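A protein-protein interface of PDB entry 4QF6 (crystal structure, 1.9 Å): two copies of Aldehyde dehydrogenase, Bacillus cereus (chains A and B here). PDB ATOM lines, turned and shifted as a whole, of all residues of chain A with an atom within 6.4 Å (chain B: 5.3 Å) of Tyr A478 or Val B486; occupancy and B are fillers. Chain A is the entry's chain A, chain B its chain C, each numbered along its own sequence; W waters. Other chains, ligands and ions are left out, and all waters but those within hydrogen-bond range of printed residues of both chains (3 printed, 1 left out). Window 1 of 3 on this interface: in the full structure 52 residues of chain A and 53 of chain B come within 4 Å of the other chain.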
ATOM      1  N   TYR A 130       9.582  16.731 -23.703  1.00  0.00           N
ATOM      2  CA  TYR A 130       8.629  15.660 -23.648  1.00  0.00           C
ATOM      3  C   TYR A 130       8.274  15.183 -25.051  1.00  0.00           C
ATOM      4  O   TYR A 130       8.304  14.002 -25.361  1.00  0.00           O
ATOM      5  CB  TYR A 130       7.410  16.101 -22.903  1.00  0.00           C
ATOM      6  CG  TYR A 130       6.277  15.112 -22.898  1.00  0.00           C
ATOM      7  CD1 TYR A 130       6.295  13.978 -22.084  1.00  0.00           C
ATOM      8  CD2 TYR A 130       5.241  15.237 -23.763  1.00  0.00           C
ATOM      9  CE1 TYR A 130       5.223  13.014 -22.121  1.00  0.00           C
ATOM     10  CE2 TYR A 130       4.169  14.356 -23.759  1.00  0.00           C
ATOM     11  CZ  TYR A 130       4.185  13.216 -22.986  1.00  0.00           C
ATOM     12  OH  TYR A 130       3.105  12.323 -22.983  1.00  0.00           O
ATOM     13  N   TYR A 131       7.896  16.130 -25.920  1.00  0.00           N
ATOM     14  CA  TYR A 131       7.620  15.808 -27.257  1.00  0.00           C
ATOM     15  C   TYR A 131       8.740  15.385 -28.116  1.00  0.00           C
ATOM     16  O   TYR A 131       8.477  14.546 -29.008  1.00  0.00           O
ATOM     17  CB  TYR A 131       6.736  16.894 -27.976  1.00  0.00           C
ATOM     18  CG  TYR A 131       5.355  16.790 -27.503  1.00  0.00           C
ATOM     19  CD1 TYR A 131       4.532  15.714 -27.891  1.00  0.00           C
ATOM     20  CD2 TYR A 131       4.812  17.748 -26.595  1.00  0.00           C
ATOM     21  CE1 TYR A 131       3.244  15.583 -27.372  1.00  0.00           C
ATOM     22  CE2 TYR A 131       3.519  17.619 -26.088  1.00  0.00           C
ATOM     23  CZ  TYR A 131       2.769  16.537 -26.474  1.00  0.00           C
ATOM     24  OH  TYR A 131       1.544  16.424 -25.965  1.00  0.00           O
ATOM     25  N   TRP A 134       8.571  11.756 -28.016  1.00  0.00           N
ATOM     26  CA  TRP A 134       7.523  11.083 -28.757  1.00  0.00           C
ATOM     27  C   TRP A 134       7.878  10.766 -30.223  1.00  0.00           C
ATOM     28  O   TRP A 134       7.257   9.832 -30.858  1.00  0.00           O
ATOM     29  CB  TRP A 134       6.201  11.876 -28.726  1.00  0.00           C
ATOM     30  CG  TRP A 134       5.337  11.481 -27.648  1.00  0.00           C
ATOM     31  CD1 TRP A 134       4.952  12.262 -26.639  1.00  0.00           C
ATOM     32  CD2 TRP A 134       4.827  10.172 -27.369  1.00  0.00           C
ATOM     33  NE1 TRP A 134       4.105  11.603 -25.794  1.00  0.00           N
ATOM     34  CE2 TRP A 134       4.056  10.282 -26.179  1.00  0.00           C
ATOM     35  CE3 TRP A 134       4.935   8.952 -27.993  1.00  0.00           C
ATOM     36  CZ2 TRP A 134       3.416   9.235 -25.609  1.00  0.00           C
ATOM     37  CZ3 TRP A 134       4.286   7.873 -27.436  1.00  0.00           C
ATOM     38  CH2 TRP A 134       3.541   7.992 -26.221  1.00  0.00           C
ATOM     39  N   ALA A 446     -15.792  17.547 -16.478  1.00  0.00           N
ATOM     40  CA  ALA A 446     -14.610  18.362 -16.772  1.00  0.00           C
ATOM     41  C   ALA A 446     -13.396  17.596 -17.254  1.00  0.00           C
ATOM     42  O   ALA A 446     -13.088  16.473 -16.755  1.00  0.00           O
ATOM     43  CB  ALA A 446     -14.274  19.162 -15.564  1.00  0.00           C
ATOM     44  N   GLY A 447     -12.646  18.225 -18.144  1.00  0.00           N
ATOM     45  CA  GLY A 447     -11.514  17.596 -18.714  1.00  0.00           C
ATOM     46  C   GLY A 447     -10.337  17.330 -17.823  1.00  0.00           C
ATOM     47  O   GLY A 447      -9.537  16.377 -18.050  1.00  0.00           O
ATOM     48  N   THR A 448     -10.144  18.187 -16.826  1.00  0.00           N
ATOM     49  CA  THR A 448      -9.135  17.922 -15.832  1.00  0.00           C
ATOM     50  C   THR A 448      -9.758  18.113 -14.460  1.00  0.00           C
ATOM     51  O   THR A 448     -10.464  19.099 -14.279  1.00  0.00           O
ATOM     52  CB  THR A 448      -7.948  18.894 -15.910  1.00  0.00           C
ATOM     53  OG1 THR A 448      -7.253  18.686 -17.127  1.00  0.00           O
ATOM     54  CG2 THR A 448      -6.968  18.727 -14.689  1.00  0.00           C
ATOM     55  N   ALA A 460       2.865  15.784 -19.865  1.00  0.00           N
ATOM     56  CA  ALA A 460       2.414  14.382 -20.016  1.00  0.00           C
ATOM     57  C   ALA A 460       0.916  14.086 -19.792  1.00  0.00           C
ATOM     58  O   ALA A 460       0.487  12.941 -20.009  1.00  0.00           O
ATOM     59  CB  ALA A 460       3.286  13.509 -19.102  1.00  0.00           C
ATOM     60  N   ALA A 461       0.137  15.071 -19.337  1.00  0.00           N
ATOM     61  CA  ALA A 461      -1.197  14.849 -18.832  1.00  0.00           C
ATOM     62  C   ALA A 461      -2.080  15.672 -19.736  1.00  0.00           C
ATOM     63  O   ALA A 461      -1.873  16.870 -19.844  1.00  0.00           O
ATOM     64  CB  ALA A 461      -1.358  15.367 -17.380  1.00  0.00           C
ATOM     65  N   PRO A 462      -3.014  15.019 -20.424  1.00  0.00           N
ATOM     66  CA  PRO A 462      -3.891  15.757 -21.299  1.00  0.00           C
ATOM     67  C   PRO A 462      -4.749  16.820 -20.676  1.00  0.00           C
ATOM     68  O   PRO A 462      -5.232  16.662 -19.544  1.00  0.00           O
ATOM     69  CB  PRO A 462      -4.812  14.688 -21.847  1.00  0.00           C
ATOM     70  CG  PRO A 462      -4.904  13.685 -20.854  1.00  0.00           C
ATOM     71  CD  PRO A 462      -3.483  13.648 -20.278  1.00  0.00           C
ATOM     72  N   GLY A 464      -8.084  19.679 -21.826  1.00  0.00           N
ATOM     73  CA  GLY A 464      -9.092  20.145 -22.802  1.00  0.00           C
ATOM     74  C   GLY A 464     -10.456  20.051 -22.284  1.00  0.00           C
ATOM     75  O   GLY A 464     -10.647  19.621 -21.175  1.00  0.00           O
ATOM     76  N   TYR A 466     -14.684  19.432 -21.852  1.00  0.00           N
ATOM     77  CA  TYR A 466     -15.967  18.853 -22.118  1.00  0.00           C
ATOM     78  C   TYR A 466     -16.930  19.941 -22.632  1.00  0.00           C
ATOM     79  O   TYR A 466     -16.653  21.112 -22.446  1.00  0.00           O
ATOM     80  CB  TYR A 466     -16.603  18.311 -20.849  1.00  0.00           C
ATOM     81  CG  TYR A 466     -16.141  16.942 -20.346  1.00  0.00           C
ATOM     82  CD1 TYR A 466     -14.804  16.605 -20.259  1.00  0.00           C
ATOM     83  CD2 TYR A 466     -17.086  16.034 -19.915  1.00  0.00           C
ATOM     84  CE1 TYR A 466     -14.402  15.395 -19.742  1.00  0.00           C
ATOM     85  CE2 TYR A 466     -16.705  14.785 -19.441  1.00  0.00           C
ATOM     86  CZ  TYR A 466     -15.386  14.482 -19.361  1.00  0.00           C
ATOM     87  OH  TYR A 466     -15.055  13.268 -18.803  1.00  0.00           O
ATOM     88  N   ARG A 473      -8.083  17.153 -27.111  1.00  0.00           N
ATOM     89  CA  ARG A 473      -7.137  17.339 -25.993  1.00  0.00           C
ATOM     90  C   ARG A 473      -5.815  17.817 -26.534  1.00  0.00           C
ATOM     91  O   ARG A 473      -5.380  17.426 -27.644  1.00  0.00           O
ATOM     92  CB  ARG A 473      -7.004  16.010 -25.205  1.00  0.00           C
ATOM     93  CG  ARG A 473      -8.360  15.558 -24.647  1.00  0.00           C
ATOM     94  CD  ARG A 473      -8.776  16.473 -23.462  1.00  0.00           C
ATOM     95  NE  ARG A 473     -10.031  16.135 -22.751  1.00  0.00           N
ATOM     96  CZ  ARG A 473     -11.235  16.515 -23.129  1.00  0.00           C
ATOM     97  NH1 ARG A 473     -11.393  17.212 -24.269  1.00  0.00           N
ATOM     98  NH2 ARG A 473     -12.309  16.174 -22.423  1.00  0.00           N
ATOM     99  N   GLU A 474      -5.141  18.657 -25.762  1.00  0.00           N
ATOM    100  CA  GLU A 474      -3.744  18.913 -25.982  1.00  0.00           C
ATOM    101  C   GLU A 474      -2.934  18.273 -24.821  1.00  0.00           C
ATOM    102  O   GLU A 474      -3.483  17.925 -23.792  1.00  0.00           O
ATOM    103  CB  GLU A 474      -3.499  20.387 -26.130  1.00  0.00           C
ATOM    104  CG  GLU A 474      -4.208  20.933 -27.348  1.00  0.00           C
ATOM    105  CD  GLU A 474      -3.935  22.437 -27.568  1.00  0.00           C
ATOM    106  OE1 GLU A 474      -3.767  23.213 -26.590  1.00  0.00           O
ATOM    107  OE2 GLU A 474      -3.840  22.810 -28.733  1.00  0.00           O
ATOM    108  N   LEU A 475      -1.617  18.233 -24.994  1.00  0.00           N
ATOM    109  CA  LEU A 475      -0.681  17.586 -24.074  1.00  0.00           C
ATOM    110  C   LEU A 475      -0.871  16.081 -24.090  1.00  0.00           C
ATOM    111  O   LEU A 475      -1.842  15.525 -24.609  1.00  0.00           O
ATOM    112  CB  LEU A 475      -0.712  18.185 -22.637  1.00  0.00           C
ATOM    113  CG  LEU A 475      -0.496  19.700 -22.567  1.00  0.00           C
ATOM    114  CD1 LEU A 475      -0.356  20.200 -21.117  1.00  0.00           C
ATOM    115  CD2 LEU A 475       0.797  20.069 -23.302  1.00  0.00           C
ATOM    116  N   GLY A 476       0.108  15.443 -23.493  1.00  0.00           N
ATOM    117  CA  GLY A 476       0.171  14.010 -23.430  1.00  0.00           C
ATOM    118  C   GLY A 476       0.283  13.299 -24.722  1.00  0.00           C
ATOM    119  O   GLY A 476       0.629  13.910 -25.736  1.00  0.00           O
ATOM    120  N   SER A 477       0.012  11.982 -24.680  1.00  0.00           N
ATOM    121  CA  SER A 477       0.026  11.177 -25.896  1.00  0.00           C
ATOM    122  C   SER A 477      -1.125  11.610 -26.796  1.00  0.00           C
ATOM    123  O   SER A 477      -1.019  11.583 -28.032  1.00  0.00           O
ATOM    124  CB  SER A 477      -0.090   9.666 -25.621  1.00  0.00           C
ATOM    125  OG  SER A 477      -1.321   9.375 -24.969  1.00  0.00           O
ATOM    126  N   TYR A 478      -2.210  11.996 -26.128  1.00  0.00           N
ATOM    127  CA  TYR A 478      -3.508  12.317 -26.743  1.00  0.00           C
ATOM    128  C   TYR A 478      -3.375  13.424 -27.805  1.00  0.00           C
ATOM    129  O   TYR A 478      -3.979  13.341 -28.892  1.00  0.00           O
ATOM    130  CB  TYR A 478      -4.514  12.694 -25.669  1.00  0.00           C
ATOM    131  CG  TYR A 478      -4.818  11.618 -24.647  1.00  0.00           C
ATOM    132  CD1 TYR A 478      -5.884  10.760 -24.867  1.00  0.00           C
ATOM    133  CD2 TYR A 478      -4.036  11.425 -23.452  1.00  0.00           C
ATOM    134  CE1 TYR A 478      -6.178   9.756 -23.987  1.00  0.00           C
ATOM    135  CE2 TYR A 478      -4.351  10.438 -22.546  1.00  0.00           C
ATOM    136  CZ  TYR A 478      -5.436   9.557 -22.838  1.00  0.00           C
ATOM    137  OH  TYR A 478      -5.824   8.546 -21.933  1.00  0.00           O
ATOM    138  N   ALA A 479      -2.516  14.402 -27.554  1.00  0.00           N
ATOM    139  CA  ALA A 479      -2.355  15.527 -28.439  1.00  0.00           C
ATOM    140  C   ALA A 479      -1.864  15.097 -29.837  1.00  0.00           C
ATOM    141  O   ALA A 479      -2.127  15.772 -30.833  1.00  0.00           O
ATOM    142  CB  ALA A 479      -1.350  16.492 -27.858  1.00  0.00           C
ATOM    143  N   LEU A 480      -1.095  14.038 -29.888  1.00  0.00           N
ATOM    144  CA  LEU A 480      -0.495  13.578 -31.151  1.00  0.00           C
ATOM    145  C   LEU A 480      -1.529  13.175 -32.090  1.00  0.00           C
ATOM    146  O   LEU A 480      -1.367  13.307 -33.321  1.00  0.00           O
ATOM    147  CB  LEU A 480       0.426  12.366 -30.882  1.00  0.00           C
ATOM    148  CG  LEU A 480       1.621  12.540 -29.938  1.00  0.00           C
ATOM    149  CD1 LEU A 480       2.210  11.219 -29.490  1.00  0.00           C
ATOM    150  CD2 LEU A 480       2.666  13.431 -30.581  1.00  0.00           C
ATOM    151  N   ASP A 481      -2.626  12.661 -31.586  1.00  0.00           N
ATOM    152  CA  ASP A 481      -3.636  12.110 -32.508  1.00  0.00           C
ATOM    153  C   ASP A 481      -4.301  13.212 -33.394  1.00  0.00           C
ATOM    154  O   ASP A 481      -4.866  12.934 -34.462  1.00  0.00           O
ATOM    155  CB  ASP A 481      -4.684  11.477 -31.688  1.00  0.00           C
ATOM    156  CG  ASP A 481      -4.179  10.180 -31.005  1.00  0.00           C
ATOM    157  OD1 ASP A 481      -3.135   9.648 -31.349  1.00  0.00           O
ATOM    158  OD2 ASP A 481      -4.881   9.763 -30.113  1.00  0.00           O
ATOM    159  N   ASN A 482      -4.309  14.444 -32.913  1.00  0.00           N
ATOM    160  CA  ASN A 482      -4.892  15.554 -33.649  1.00  0.00           C
ATOM    161  C   ASN A 482      -4.105  15.892 -34.886  1.00  0.00           C
ATOM    162  O   ASN A 482      -4.641  16.513 -35.815  1.00  0.00           O
ATOM    163  CB  ASN A 482      -4.880  16.839 -32.848  1.00  0.00           C
ATOM    164  CG  ASN A 482      -5.617  16.740 -31.507  1.00  0.00           C
ATOM    165  OD1 ASN A 482      -5.137  17.261 -30.513  1.00  0.00           O
ATOM    166  ND2 ASN A 482      -6.711  16.037 -31.467  1.00  0.00           N
ATOM    167  N   GLY B 140      -7.751   3.731 -19.826  1.00  0.00           N
ATOM    168  CA  GLY B 140      -6.992   4.985 -19.793  1.00  0.00           C
ATOM    169  C   GLY B 140      -5.645   4.749 -19.276  1.00  0.00           C
ATOM    170  O   GLY B 140      -5.163   3.555 -19.264  1.00  0.00           O
ATOM    171  N   GLN B 141      -4.993   5.810 -18.827  1.00  0.00           N
ATOM    172  CA  GLN B 141      -3.580   5.739 -18.497  1.00  0.00           C
ATOM    173  C   GLN B 141      -3.279   6.072 -17.030  1.00  0.00           C
ATOM    174  O   GLN B 141      -3.980   6.867 -16.442  1.00  0.00           O
ATOM    175  CB  GLN B 141      -2.824   6.777 -19.376  1.00  0.00           C
ATOM    176  CG  GLN B 141      -2.990   6.599 -20.880  1.00  0.00           C
ATOM    177  CD  GLN B 141      -2.141   7.638 -21.676  1.00  0.00           C
ATOM    178  OE1 GLN B 141      -1.447   8.490 -21.108  1.00  0.00           O
ATOM    179  NE2 GLN B 141      -2.232   7.575 -22.956  1.00  0.00           N
ATOM    180  N   THR B 153      -5.973   8.936 -16.297  1.00  0.00           N
ATOM    181  CA  THR B 153      -7.065   9.305 -17.152  1.00  0.00           C
ATOM    182  C   THR B 153      -8.203   8.279 -17.148  1.00  0.00           C
ATOM    183  O   THR B 153      -8.020   7.056 -16.917  1.00  0.00           O
ATOM    184  CB  THR B 153      -6.595   9.641 -18.553  1.00  0.00           C
ATOM    185  OG1 THR B 153      -6.081   8.441 -19.171  1.00  0.00           O
ATOM    186  CG2 THR B 153      -5.485  10.710 -18.477  1.00  0.00           C
ATOM    187  N   ARG B 154      -9.384   8.797 -17.426  1.00  0.00           N
ATOM    188  CA  ARG B 154     -10.614   7.976 -17.628  1.00  0.00           C
ATOM    189  C   ARG B 154     -11.118   8.286 -18.987  1.00  0.00           C
ATOM    190  O   ARG B 154     -11.139   9.420 -19.354  1.00  0.00           O
ATOM    191  CB  ARG B 154     -11.727   8.424 -16.676  1.00  0.00           C
ATOM    192  CG  ARG B 154     -11.582   7.834 -15.306  1.00  0.00           C
ATOM    193  CD  ARG B 154     -12.403   8.514 -14.239  1.00  0.00           C
ATOM    194  NE  ARG B 154     -13.798   8.702 -14.510  1.00  0.00           N
ATOM    195  CZ  ARG B 154     -14.783   7.848 -14.282  1.00  0.00           C
ATOM    196  NH1 ARG B 154     -14.592   6.635 -13.822  1.00  0.00           N
ATOM    197  NH2 ARG B 154     -15.998   8.252 -14.495  1.00  0.00           N
ATOM    198  N   HIS B 155     -11.539   7.256 -19.738  1.00  0.00           N
ATOM    199  CA  HIS B 155     -12.122   7.450 -21.035  1.00  0.00           C
ATOM    200  C   HIS B 155     -13.596   7.266 -20.840  1.00  0.00           C
ATOM    201  O   HIS B 155     -14.095   6.165 -20.905  1.00  0.00           O
ATOM    202  CB  HIS B 155     -11.515   6.454 -22.025  1.00  0.00           C
ATOM    203  CG  HIS B 155     -10.057   6.687 -22.290  1.00  0.00           C
ATOM    204  ND1 HIS B 155      -9.440   6.255 -23.433  1.00  0.00           N
ATOM    205  CD2 HIS B 155      -9.126   7.396 -21.615  1.00  0.00           C
ATOM    206  CE1 HIS B 155      -8.171   6.607 -23.419  1.00  0.00           C
ATOM    207  NE2 HIS B 155      -7.958   7.330 -22.338  1.00  0.00           N
ATOM    208  N   GLU B 156     -14.274   8.354 -20.570  1.00  0.00           N
ATOM    209  CA  GLU B 156     -15.678   8.329 -20.174  1.00  0.00           C
ATOM    210  C   GLU B 156     -16.535   8.325 -21.423  1.00  0.00           C
ATOM    211  O   GLU B 156     -16.172   8.970 -22.357  1.00  0.00           O
ATOM    212  CB  GLU B 156     -16.060   9.557 -19.365  1.00  0.00           C
ATOM    213  CG  GLU B 156     -15.307   9.598 -18.058  1.00  0.00           C
ATOM    214  CD  GLU B 156     -15.780  10.700 -17.119  1.00  0.00           C
ATOM    215  OE1 GLU B 156     -16.514  11.636 -17.548  1.00  0.00           O
ATOM    216  OE2 GLU B 156     -15.436  10.605 -15.946  1.00  0.00           O
ATOM    217  N   THR B 484     -15.649   8.826 -26.656  1.00  0.00           N
ATOM    218  CA  THR B 484     -15.278   9.093 -25.298  1.00  0.00           C
ATOM    219  C   THR B 484     -14.814  10.546 -25.071  1.00  0.00           C
ATOM    220  O   THR B 484     -14.393  11.192 -25.997  1.00  0.00           O
ATOM    221  CB  THR B 484     -14.208   8.111 -24.828  1.00  0.00           C
ATOM    222  OG1 THR B 484     -13.063   8.255 -25.627  1.00  0.00           O
ATOM    223  CG2 THR B 484     -14.657   6.726 -24.954  1.00  0.00           C
ATOM    224  N   GLU B 485     -14.952  11.054 -23.850  1.00  0.00           N
ATOM    225  CA  GLU B 485     -14.271  12.242 -23.395  1.00  0.00           C
ATOM    226  C   GLU B 485     -13.192  11.803 -22.409  1.00  0.00           C
ATOM    227  O   GLU B 485     -13.454  10.948 -21.599  1.00  0.00           O
ATOM    228  CB  GLU B 485     -15.191  13.120 -22.591  1.00  0.00           C
ATOM    229  CG  GLU B 485     -16.171  13.955 -23.390  1.00  0.00           C
ATOM    230  CD  GLU B 485     -15.660  15.112 -24.173  1.00  0.00           C
ATOM    231  OE1 GLU B 485     -16.519  15.674 -24.911  1.00  0.00           O
ATOM    232  OE2 GLU B 485     -14.468  15.447 -24.155  1.00  0.00           O
ATOM    233  N   VAL B 486     -12.005  12.378 -22.529  1.00  0.00           N
ATOM    234  CA  VAL B 486     -10.882  12.028 -21.756  1.00  0.00           C
ATOM    235  C   VAL B 486     -10.775  12.973 -20.561  1.00  0.00           C
ATOM    236  O   VAL B 486     -10.878  14.218 -20.685  1.00  0.00           O
ATOM    237  CB  VAL B 486      -9.548  12.174 -22.552  1.00  0.00           C
ATOM    238  CG1 VAL B 486      -8.323  12.000 -21.640  1.00  0.00           C
ATOM    239  CG2 VAL B 486      -9.467  11.211 -23.701  1.00  0.00           C
ATOM    240  N   LYS B 487     -10.684  12.357 -19.380  1.00  0.00           N
ATOM    241  CA  LYS B 487     -10.661  13.149 -18.170  1.00  0.00           C
ATOM    242  C   LYS B 487      -9.353  12.849 -17.496  1.00  0.00           C
ATOM    243  O   LYS B 487      -9.085  11.688 -17.259  1.00  0.00           O
ATOM    244  CB  LYS B 487     -11.778  12.768 -17.226  1.00  0.00           C
ATOM    245  CG  LYS B 487     -11.608  13.424 -15.852  1.00  0.00           C
ATOM    246  CD  LYS B 487     -12.754  13.087 -14.908  1.00  0.00           C
ATOM    247  CE  LYS B 487     -14.120  13.730 -15.346  1.00  0.00           C
ATOM    248  NZ  LYS B 487     -15.266  13.160 -14.501  1.00  0.00           N
ATOM    249  N   SER B 488      -8.562  13.873 -17.259  1.00  0.00           N
ATOM    250  CA  SER B 488      -7.297  13.752 -16.540  1.00  0.00           C
ATOM    251  C   SER B 488      -7.467  14.038 -15.067  1.00  0.00           C
ATOM    252  O   SER B 488      -7.843  15.165 -14.643  1.00  0.00           O
ATOM    253  CB  SER B 488      -6.320  14.688 -17.227  1.00  0.00           C
ATOM    254  OG  SER B 488      -5.117  14.887 -16.582  1.00  0.00           O
HETATM  255  O   HOH W   1     -11.693  13.986 -24.842  1.00  0.00           O
HETATM  256  O   HOH W   2      -0.845  11.210 -21.822  1.00  0.00           O
HETATM  257  O   HOH W   3      -4.660  17.571 -17.017  1.00  0.00           O
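O of Gly A447 lies within hydrogen-bond range of N of Ser B488 (2.8 Å).
The side-chain hydroxyl (OG) of Ser B488 lies close to the backbone carbonyl oxygen (O) of Pro A462.
The side-chain hydroxyl of Tyr A466 lies within hydrogen-bond range of the side-chain carboxylate of Glu B156 (2.5 Å).
The guanidinium group (NH2) of Arg A473 is in salt-bridge range of the side-chain carboxylate (OE2) of Glu B485 (2.9 Å).
The guanidinium group (NE) of Arg A473 is in hydrogen-bond range of the backbone carbonyl oxygen (O) of Val B486 (2.9 Å).
The side-chain hydroxyl of Ser A477 is in hydrogen-bond range of the side-chain amide nitrogen of Gln B141.
OH of Tyr A478 is in hydrogen-bond range of OG1 of Thr B153, 2.8 Å away.
The side-chain hydroxyl of Tyr A478 sits at hydrogen-bond distance from a ring nitrogen (NE2) of His B155 (2.5 Å).
The side-chain amide oxygen (OD1) of Asn A482 sits close to the backbone carbonyl oxygen (O) of Arg A473.
The side-chain hydroxyl (OG1) of Thr B153 lies within hydrogen-bond range of the backbone NH (N) of Gln B141 (2.9 Å).
NH2 of Arg B154 is in salt-bridge range of OE2 of Glu B156 (2.8 Å).
The backbone NH of Arg B154 is in hydrogen-bond range of the backbone carbonyl oxygen of Lys B487.
The backbone NH (N) of Glu B485 lies within hydrogen-bond range of the backbone carbonyl oxygen (O) of Glu B156 (2.8 Å).
The side-chain amino group of Lys B487 lies within salt-bridge range of the side-chain carboxylate of Glu B156 (2.9 Å).
Ala A446 touches Lys B487 (O to CE, 3.3 Å).
Lys B487 touches Gly A447 (CA to O, 3.4 Å).
CA of Thr A448 touches O of Ser B488 (3.3 Å).
Ser B488 touches Ala A461.
Pro A462 touches Thr B153 (CG to CG2, 3.9 Å).
CG of Pro A462 touches CG1 of Val B486 (3.9 Å).
CZ of Tyr A466 touches CB of Glu B485, at 3.5 Å.
Tyr A466 touches Val B486.
Lys B487 touches Tyr A466 (CE to OH, 3.6 Å).
Val B486 touches Tyr A478 (CG2 to CE1, 3.6 Å).
Of the printed residues of chain B, Gly A447 touches Val B486, Lys B487 and Ser B488.
Of the printed residues of chain B, Thr A448 touches Ser B488.
Of chain B, only Gln B141, Thr B153, His B155 and Val B486 come within 4 Å of Tyr A478.
Thr B484 touches none of the printed residues of chain A.
Printed residues of chain A that touch a printed residue of chain B: Ala A446, Gly A447, Thr A448, Ala A461, Pro A462, Tyr A466, Arg A473, Ser A477 and Tyr A478.
Hydrophobic or aromatic side chains of chain A that line the printed part of chain B: Ala A461, Pro A462, Tyr A466 and Tyr A478.
Of the 11 printed residues of chain B, 8 touch a printed residue of chain A.
Hydrophobic or aromatic side chains of chain B that line the printed part of chain A: His B155 and Val B486.
Along chain B the printed residues that touch a printed residue of chain A span positions 141 to 488.
Among the printed residues, 20 pairs touch across the chains.
No position is printed for both chains.
Of the 20 pairs that touch across the chains among the printed residues, none has its exchanged pair printed and touching as well.
Water W3 lies within hydrogen-bond range of the backbone carbonyl oxygen (O) of Pro A462, the side-chain hydroxyl (OG) of Ser B488 and the side-chain hydroxyl (OG1) of Thr A448.
Water W1 lies within hydrogen-bond range of N of Val B486 (2.8 Å), OE2 of Glu B485 (3.2 Å) and NH1 of Arg A473 (3.3 Å).
Water W2 lies within hydrogen-bond range of O of Ala A460 (2.8 Å), OE1 of Gln B141 (2.9 Å) and N of Ser A477 (3.1 Å).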
